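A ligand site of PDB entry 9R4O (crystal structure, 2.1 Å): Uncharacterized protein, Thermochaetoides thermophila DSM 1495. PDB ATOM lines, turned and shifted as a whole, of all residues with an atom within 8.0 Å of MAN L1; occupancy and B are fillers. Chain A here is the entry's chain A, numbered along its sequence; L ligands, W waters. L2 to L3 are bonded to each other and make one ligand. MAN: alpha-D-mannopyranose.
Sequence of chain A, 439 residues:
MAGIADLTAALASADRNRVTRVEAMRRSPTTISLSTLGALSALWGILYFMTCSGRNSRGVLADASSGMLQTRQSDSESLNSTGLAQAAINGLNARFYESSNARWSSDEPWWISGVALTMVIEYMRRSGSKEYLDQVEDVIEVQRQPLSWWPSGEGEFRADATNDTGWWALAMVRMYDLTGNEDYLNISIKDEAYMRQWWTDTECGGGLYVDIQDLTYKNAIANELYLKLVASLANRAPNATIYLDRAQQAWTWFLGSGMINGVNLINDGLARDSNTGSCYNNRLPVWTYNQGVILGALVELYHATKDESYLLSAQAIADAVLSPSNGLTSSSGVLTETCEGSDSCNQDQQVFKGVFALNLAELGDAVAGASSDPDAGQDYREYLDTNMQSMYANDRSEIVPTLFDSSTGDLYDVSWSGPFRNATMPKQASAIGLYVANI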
ATOM      1  N   ARG A 103       2.514  10.301   6.213  1.00  0.00           N
ATOM      2  CA  ARG A 103       2.858  11.054   7.400  1.00  0.00           C
ATOM      3  C   ARG A 103       4.220  10.594   7.901  1.00  0.00           C
ATOM      4  O   ARG A 103       4.605   9.438   7.703  1.00  0.00           O
ATOM      5  CB  ARG A 103       1.777  10.875   8.491  1.00  0.00           C
ATOM      6  CG  ARG A 103       2.302  10.812   9.907  1.00  0.00           C
ATOM      7  CD  ARG A 103       1.185  10.892  10.929  1.00  0.00           C
ATOM      8  NE  ARG A 103       1.646  11.477  12.187  1.00  0.00           N
ATOM      9  CZ  ARG A 103       0.883  11.662  13.256  1.00  0.00           C
ATOM     10  NH1 ARG A 103      -0.393  11.304  13.254  1.00  0.00           N
ATOM     11  NH2 ARG A 103       1.408  12.209  14.343  1.00  0.00           N
ATOM     12  N   SER A 105       6.354   9.668  11.094  1.00  0.00           N
ATOM     13  CA  SER A 105       6.378   9.292  12.505  1.00  0.00           C
ATOM     14  C   SER A 105       5.046   9.492  13.212  1.00  0.00           C
ATOM     15  O   SER A 105       4.832  10.517  13.860  1.00  0.00           O
ATOM     16  CB  SER A 105       7.468  10.077  13.236  1.00  0.00           C
ATOM     17  OG  SER A 105       8.765   9.598  12.906  1.00  0.00           O
ATOM     18  N   SER A 106       4.148   8.510  13.115  1.00  0.00           N
ATOM     19  CA  SER A 106       2.862   8.604  13.797  1.00  0.00           C
ATOM     20  C   SER A 106       3.013   8.627  15.309  1.00  0.00           C
ATOM     21  O   SER A 106       2.080   9.054  16.006  1.00  0.00           O
ATOM     22  CB  SER A 106       1.948   7.446  13.375  1.00  0.00           C
ATOM     23  OG  SER A 106       1.589   7.555  12.004  1.00  0.00           O
ATOM     24  N   ASP A 107       4.152   8.184  15.835  1.00  0.00           N
ATOM     25  CA  ASP A 107       4.395   8.215  17.268  1.00  0.00           C
ATOM     26  C   ASP A 107       4.864   9.574  17.775  1.00  0.00           C
ATOM     27  O   ASP A 107       4.986   9.757  18.993  1.00  0.00           O
ATOM     28  CB  ASP A 107       5.433   7.134  17.635  1.00  0.00           C
ATOM     29  CG  ASP A 107       6.771   7.356  16.956  1.00  0.00           C
ATOM     30  OD1 ASP A 107       6.866   8.238  16.072  1.00  0.00           O
ATOM     31  OD2 ASP A 107       7.727   6.630  17.283  1.00  0.00           O
ATOM     32  N   GLU A 108       5.118  10.519  16.886  1.00  0.00           N
ATOM     33  CA  GLU A 108       5.534  11.867  17.244  1.00  0.00           C
ATOM     34  C   GLU A 108       4.410  12.872  16.974  1.00  0.00           C
ATOM     35  O   GLU A 108       3.501  12.588  16.199  1.00  0.00           O
ATOM     36  CB  GLU A 108       6.804  12.253  16.461  1.00  0.00           C
ATOM     37  CG  GLU A 108       7.916  11.227  16.608  1.00  0.00           C
ATOM     38  CD  GLU A 108       8.887  11.574  17.735  1.00  0.00           C
ATOM     39  OE1 GLU A 108       8.423  11.820  18.865  1.00  0.00           O
ATOM     40  OE2 GLU A 108      10.114  11.566  17.495  1.00  0.00           O
ATOM     41  N   PRO A 109       4.444  14.035  17.632  1.00  0.00           N
ATOM     42  CA  PRO A 109       3.331  14.985  17.510  1.00  0.00           C
ATOM     43  C   PRO A 109       2.934  15.268  16.061  1.00  0.00           C
ATOM     44  O   PRO A 109       3.781  15.418  15.182  1.00  0.00           O
ATOM     45  CB  PRO A 109       3.861  16.248  18.193  1.00  0.00           C
ATOM     46  CG  PRO A 109       5.083  15.844  18.963  1.00  0.00           C
ATOM     47  CD  PRO A 109       5.395  14.404  18.691  1.00  0.00           C
ATOM     48  N   TRP A 110       1.618  15.337  15.839  1.00  0.00           N
ATOM     49  CA  TRP A 110       1.100  15.542  14.488  1.00  0.00           C
ATOM     50  C   TRP A 110       1.544  16.885  13.920  1.00  0.00           C
ATOM     51  O   TRP A 110       1.827  17.001  12.728  1.00  0.00           O
ATOM     52  CB  TRP A 110      -0.422  15.436  14.503  1.00  0.00           C
ATOM     53  CG  TRP A 110      -1.084  15.663  13.169  1.00  0.00           C
ATOM     54  CD1 TRP A 110      -1.082  14.822  12.094  1.00  0.00           C
ATOM     55  CD2 TRP A 110      -1.866  16.802  12.780  1.00  0.00           C
ATOM     56  NE1 TRP A 110      -1.800  15.361  11.068  1.00  0.00           N
ATOM     57  CE2 TRP A 110      -2.297  16.574  11.452  1.00  0.00           C
ATOM     58  CE3 TRP A 110      -2.237  17.989  13.425  1.00  0.00           C
ATOM     59  CZ2 TRP A 110      -3.080  17.503  10.765  1.00  0.00           C
ATOM     60  CZ3 TRP A 110      -3.024  18.896  12.735  1.00  0.00           C
ATOM     61  CH2 TRP A 110      -3.440  18.651  11.414  1.00  0.00           C
ATOM     62  N   TRP A 111       1.636  17.915  14.769  1.00  0.00           N
ATOM     63  CA  TRP A 111       2.020  19.231  14.277  1.00  0.00           C
ATOM     64  C   TRP A 111       3.455  19.266  13.766  1.00  0.00           C
ATOM     65  O   TRP A 111       3.800  20.153  12.982  1.00  0.00           O
ATOM     66  CB  TRP A 111       1.820  20.288  15.373  1.00  0.00           C
ATOM     67  CG  TRP A 111       2.771  20.195  16.526  1.00  0.00           C
ATOM     68  CD1 TRP A 111       2.618  19.441  17.650  1.00  0.00           C
ATOM     69  CD2 TRP A 111       4.009  20.912  16.694  1.00  0.00           C
ATOM     70  NE1 TRP A 111       3.678  19.623  18.501  1.00  0.00           N
ATOM     71  CE2 TRP A 111       4.548  20.527  17.937  1.00  0.00           C
ATOM     72  CE3 TRP A 111       4.705  21.829  15.908  1.00  0.00           C
ATOM     73  CZ2 TRP A 111       5.761  21.022  18.420  1.00  0.00           C
ATOM     74  CZ3 TRP A 111       5.904  22.331  16.386  1.00  0.00           C
ATOM     75  CH2 TRP A 111       6.416  21.923  17.629  1.00  0.00           C
ATOM     76  N   ILE A 112       4.292  18.317  14.194  1.00  0.00           N
ATOM     77  CA  ILE A 112       5.671  18.303  13.712  1.00  0.00           C
ATOM     78  C   ILE A 112       5.733  17.733  12.297  1.00  0.00           C
ATOM     79  O   ILE A 112       6.628  18.099  11.517  1.00  0.00           O
ATOM     80  CB  ILE A 112       6.578  17.541  14.689  1.00  0.00           C
ATOM     81  CG1 ILE A 112       6.374  18.080  16.112  1.00  0.00           C
ATOM     82  CG2 ILE A 112       8.041  17.676  14.277  1.00  0.00           C
ATOM     83  CD1 ILE A 112       7.562  17.908  17.036  1.00  0.00           C
ATOM     84  N   SER A 113       4.795  16.847  11.933  1.00  0.00           N
ATOM     85  CA  SER A 113       4.648  16.488  10.522  1.00  0.00           C
ATOM     86  C   SER A 113       4.365  17.730   9.676  1.00  0.00           C
ATOM     87  O   SER A 113       4.886  17.857   8.567  1.00  0.00           O
ATOM     88  CB  SER A 113       3.523  15.467  10.344  1.00  0.00           C
ATOM     89  OG  SER A 113       3.990  14.152  10.592  1.00  0.00           O
ATOM     90  N   LEU A 147      -9.762  14.848  10.994  1.00  0.00           N
ATOM     91  CA  LEU A 147      -8.915  14.136  11.947  1.00  0.00           C
ATOM     92  C   LEU A 147      -9.757  13.220  12.823  1.00  0.00           C
ATOM     93  O   LEU A 147     -10.838  13.586  13.289  1.00  0.00           O
ATOM     94  CB  LEU A 147      -8.133  15.124  12.804  1.00  0.00           C
ATOM     95  CG  LEU A 147      -7.411  16.203  11.999  1.00  0.00           C
ATOM     96  CD1 LEU A 147      -6.743  17.207  12.919  1.00  0.00           C
ATOM     97  CD2 LEU A 147      -6.389  15.568  11.066  1.00  0.00           C
ATOM     98  N   SER A 148      -9.248  12.006  13.048  1.00  0.00           N
ATOM     99  CA  SER A 148      -9.973  11.034  13.871  1.00  0.00           C
ATOM    100  C   SER A 148     -10.113  11.509  15.308  1.00  0.00           C
ATOM    101  O   SER A 148     -11.093  11.160  15.978  1.00  0.00           O
ATOM    102  CB  SER A 148      -9.271   9.685  13.827  1.00  0.00           C
ATOM    103  OG  SER A 148      -7.858   9.836  13.824  1.00  0.00           O
ATOM    104  N   TRP A 149      -9.164  12.297  15.809  1.00  0.00           N
ATOM    105  CA  TRP A 149      -9.216  12.793  17.177  1.00  0.00           C
ATOM    106  C   TRP A 149      -9.894  14.151  17.291  1.00  0.00           C
ATOM    107  O   TRP A 149     -10.042  14.659  18.407  1.00  0.00           O
ATOM    108  CB  TRP A 149      -7.808  12.866  17.769  1.00  0.00           C
ATOM    109  CG  TRP A 149      -6.887  13.816  17.079  1.00  0.00           C
ATOM    110  CD1 TRP A 149      -6.663  15.129  17.406  1.00  0.00           C
ATOM    111  CD2 TRP A 149      -6.045  13.543  15.958  1.00  0.00           C
ATOM    112  NE1 TRP A 149      -5.748  15.682  16.542  1.00  0.00           N
ATOM    113  CE2 TRP A 149      -5.343  14.726  15.650  1.00  0.00           C
ATOM    114  CE3 TRP A 149      -5.804  12.406  15.186  1.00  0.00           C
ATOM    115  CZ2 TRP A 149      -4.430  14.809  14.607  1.00  0.00           C
ATOM    116  CZ3 TRP A 149      -4.897  12.487  14.135  1.00  0.00           C
ATOM    117  CH2 TRP A 149      -4.222  13.685  13.855  1.00  0.00           C
ATOM    118  N   TRP A 150     -10.308  14.753  16.170  1.00  0.00           N
ATOM    119  CA  TRP A 150     -11.054  16.021  16.195  1.00  0.00           C
ATOM    120  C   TRP A 150     -11.939  16.099  14.963  1.00  0.00           C
ATOM    121  O   TRP A 150     -11.673  16.857  14.023  1.00  0.00           O
ATOM    122  CB  TRP A 150     -10.100  17.210  16.277  1.00  0.00           C
ATOM    123  CG  TRP A 150     -10.797  18.485  16.644  1.00  0.00           C
ATOM    124  CD1 TRP A 150     -10.964  19.587  15.862  1.00  0.00           C
ATOM    125  CD2 TRP A 150     -11.440  18.787  17.894  1.00  0.00           C
ATOM    126  NE1 TRP A 150     -11.655  20.560  16.545  1.00  0.00           N
ATOM    127  CE2 TRP A 150     -11.966  20.093  17.792  1.00  0.00           C
ATOM    128  CE3 TRP A 150     -11.617  18.079  19.084  1.00  0.00           C
ATOM    129  CZ2 TRP A 150     -12.650  20.702  18.836  1.00  0.00           C
ATOM    130  CZ3 TRP A 150     -12.300  18.688  20.128  1.00  0.00           C
ATOM    131  CH2 TRP A 150     -12.813  19.987  19.993  1.00  0.00           C
ATOM    132  N   ALA A 159      -7.780  21.390  13.849  1.00  0.00           N
ATOM    133  CA  ALA A 159      -7.488  20.410  14.871  1.00  0.00           C
ATOM    134  C   ALA A 159      -7.998  20.859  16.247  1.00  0.00           C
ATOM    135  O   ALA A 159      -8.731  21.851  16.362  1.00  0.00           O
ATOM    136  CB  ALA A 159      -5.977  20.135  14.907  1.00  0.00           C
ATOM    137  N   ASP A 160      -7.617  20.119  17.283  1.00  0.00           N
ATOM    138  CA  ASP A 160      -8.063  20.365  18.653  1.00  0.00           C
ATOM    139  C   ASP A 160      -7.197  21.378  19.380  1.00  0.00           C
ATOM    140  O   ASP A 160      -7.441  21.646  20.564  1.00  0.00           O
ATOM    141  CB  ASP A 160      -8.087  19.052  19.446  1.00  0.00           C
ATOM    142  CG  ASP A 160      -6.748  18.333  19.425  1.00  0.00           C
ATOM    143  OD1 ASP A 160      -5.821  18.796  18.733  1.00  0.00           O
ATOM    144  OD2 ASP A 160      -6.624  17.297  20.116  1.00  0.00           O
ATOM    145  N   ALA A 161      -6.188  21.941  18.725  1.00  0.00           N
ATOM    146  CA  ALA A 161      -5.360  22.996  19.302  1.00  0.00           C
ATOM    147  C   ALA A 161      -5.042  23.999  18.211  1.00  0.00           C
ATOM    148  O   ALA A 161      -4.678  23.604  17.097  1.00  0.00           O
ATOM    149  CB  ALA A 161      -4.075  22.423  19.917  1.00  0.00           C
ATOM    150  N   ASP A 164      -1.659  23.603  16.483  1.00  0.00           N
ATOM    151  CA  ASP A 164      -1.604  22.537  15.479  1.00  0.00           C
ATOM    152  C   ASP A 164      -2.118  23.033  14.134  1.00  0.00           C
ATOM    153  O   ASP A 164      -1.472  22.824  13.092  1.00  0.00           O
ATOM    154  CB  ASP A 164      -2.409  21.323  15.944  1.00  0.00           C
ATOM    155  CG  ASP A 164      -1.815  20.656  17.160  1.00  0.00           C
ATOM    156  OD1 ASP A 164      -1.041  21.320  17.885  1.00  0.00           O
ATOM    157  OD2 ASP A 164      -2.113  19.467  17.388  1.00  0.00           O
ATOM    158  N   GLN A 213     -10.175  22.967  23.767  1.00  0.00           N
ATOM    159  CA  GLN A 213     -11.123  22.268  24.637  1.00  0.00           C
ATOM    160  C   GLN A 213     -11.256  22.953  26.003  1.00  0.00           C
ATOM    161  O   GLN A 213     -12.320  22.864  26.624  1.00  0.00           O
ATOM    162  CB  GLN A 213     -10.691  20.817  24.813  1.00  0.00           C
ATOM    163  CG  GLN A 213     -10.474  20.071  23.508  1.00  0.00           C
ATOM    164  CD  GLN A 213     -10.675  18.579  23.649  1.00  0.00           C
ATOM    165  OE1 GLN A 213      -9.760  17.791  23.418  1.00  0.00           O
ATOM    166  NE2 GLN A 213     -11.882  18.171  24.042  1.00  0.00           N
ATOM    167  N   GLN A 347       9.933  15.734  22.784  1.00  0.00           N
ATOM    168  CA  GLN A 347       9.659  15.607  21.352  1.00  0.00           C
ATOM    169  C   GLN A 347       9.336  16.966  20.738  1.00  0.00           C
ATOM    170  O   GLN A 347       9.773  17.257  19.610  1.00  0.00           O
ATOM    171  CB  GLN A 347       8.507  14.625  21.130  1.00  0.00           C
ATOM    172  CG  GLN A 347       7.376  14.729  22.129  1.00  0.00           C
ATOM    173  CD  GLN A 347       6.465  13.509  22.115  1.00  0.00           C
ATOM    174  OE1 GLN A 347       6.806  12.479  21.530  1.00  0.00           O
ATOM    175  NE2 GLN A 347       5.314  13.625  22.759  1.00  0.00           N
ATOM    176  N   ASP A 348       8.598  17.819  21.454  1.00  0.00           N
ATOM    177  CA  ASP A 348       8.290  19.153  20.938  1.00  0.00           C
ATOM    178  C   ASP A 348       9.559  19.991  20.796  1.00  0.00           C
ATOM    179  O   ASP A 348       9.841  20.528  19.712  1.00  0.00           O
ATOM    180  CB  ASP A 348       7.280  19.844  21.845  1.00  0.00           C
ATOM    181  CG  ASP A 348       5.984  19.072  21.974  1.00  0.00           C
ATOM    182  OD1 ASP A 348       5.570  18.798  23.117  1.00  0.00           O
ATOM    183  OD2 ASP A 348       5.363  18.756  20.931  1.00  0.00           O
HETATM  184  C1  MAN L   1      -3.363  14.611  19.769  1.00  0.00           C
HETATM  185  C2  MAN L   1      -2.023  15.182  19.282  1.00  0.00           C
HETATM  186  C3  MAN L   1      -1.571  14.476  18.014  1.00  0.00           C
HETATM  187  C4  MAN L   1      -1.849  12.966  18.114  1.00  0.00           C
HETATM  188  C5  MAN L   1      -3.369  12.719  18.222  1.00  0.00           C
HETATM  189  C6  MAN L   1      -3.736  11.508  19.085  1.00  0.00           C
HETATM  190  O1  MAN L   1      -4.124  15.706  20.224  1.00  0.00           O
HETATM  191  O2  MAN L   1      -0.986  14.964  20.237  1.00  0.00           O
HETATM  192  O3  MAN L   1      -0.196  14.712  17.746  1.00  0.00           O
HETATM  193  O4  MAN L   1      -1.337  12.306  16.966  1.00  0.00           O
HETATM  194  O5  MAN L   1      -4.046  13.877  18.775  1.00  0.00           O
HETATM  195  O6  MAN L   1      -3.146  10.343  18.493  1.00  0.00           O
HETATM  196  C1  MAN L   2       0.260  21.879  21.827  1.00  0.00           C
HETATM  197  C2  MAN L   2      -0.117  20.520  21.206  1.00  0.00           C
HETATM  198  C3  MAN L   2       0.654  19.396  21.862  1.00  0.00           C
HETATM  199  C4  MAN L   2       2.118  19.787  22.013  1.00  0.00           C
HETATM  200  C5  MAN L   2       2.240  20.957  22.998  1.00  0.00           C
HETATM  201  C6  MAN L   2       3.457  21.844  22.737  1.00  0.00           C
HETATM  202  O1  MAN L   2      -0.971  22.528  22.071  1.00  0.00           O
HETATM  203  O2  MAN L   2       0.227  20.478  19.819  1.00  0.00           O
HETATM  204  O3  MAN L   2       0.551  18.187  21.127  1.00  0.00           O
HETATM  205  O4  MAN L   2       2.868  18.693  22.510  1.00  0.00           O
HETATM  206  O5  MAN L   2       1.026  21.778  23.012  1.00  0.00           O
HETATM  207  O6  MAN L   2       3.203  23.159  23.235  1.00  0.00           O
HETATM  208  C1  MAN L   3       3.386  23.215  24.665  1.00  0.00           C
HETATM  209  C2  MAN L   3       2.845  24.585  25.107  1.00  0.00           C
HETATM  210  C3  MAN L   3       3.741  25.678  24.541  1.00  0.00           C
HETATM  211  C4  MAN L   3       5.209  25.453  24.919  1.00  0.00           C
HETATM  212  C5  MAN L   3       5.680  24.042  24.539  1.00  0.00           C
HETATM  213  C6  MAN L   3       7.050  23.713  25.107  1.00  0.00           C
HETATM  214  O2  MAN L   3       2.881  24.729  26.524  1.00  0.00           O
HETATM  215  O3  MAN L   3       3.320  26.972  24.974  1.00  0.00           O
HETATM  216  O4  MAN L   3       6.025  26.410  24.251  1.00  0.00           O
HETATM  217  O5  MAN L   3       4.743  23.056  25.050  1.00  0.00           O
HETATM  218  O6  MAN L   3       7.320  22.337  24.856  1.00  0.00           O
HETATM  219  O   HOH W   1       0.054  17.572  17.345  1.00  0.00           O
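NE1 of Trp 149 lies close to O5 of MAN L1 (3.3 Å).
An oxygen (O3) of MAN L1 lies within hydrogen-bond range of the backbone NH (N) of Trp 110, 2.7 Å away.
OD2 of Asp 160 lies within hydrogen-bond range of O1 of MAN L1 (3.0 Å).
OD1 of Asp 164 sits at hydrogen-bond distance from O2 of MAN L2, 2.5 Å away.
The side-chain carboxylate (OD1) of Asp 348 is in hydrogen-bond range of an oxygen (O4) of MAN L2 (2.8 Å).
The guanidinium group (NH2) of Arg 103 lies within hydrogen-bond range of the backbone carbonyl oxygen (O) of Glu 108 (2.8 Å).
Arg 103 touches MAN L1 (NH2 to O4, 3.8 Å).
Pro 109 touches MAN L1.
Hydrophobic or aromatic side chains that line MAN L1: Trp 110 and Trp 149.
Of the 21 residues printed, 5 come within 4 Å of MAN L1.
The nearest printed residue that does not touch MAN L1 is Glu 108 (4.5 Å).
Water W1 lies within hydrogen-bond range of the side-chain carboxylate of Asp 164 (2.9 Å), an oxygen (O3) of MAN L1 (2.9 Å), the backbone NH of Trp 111 (3.0 Å) and the backbone NH of Trp 110 (3.1 Å).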
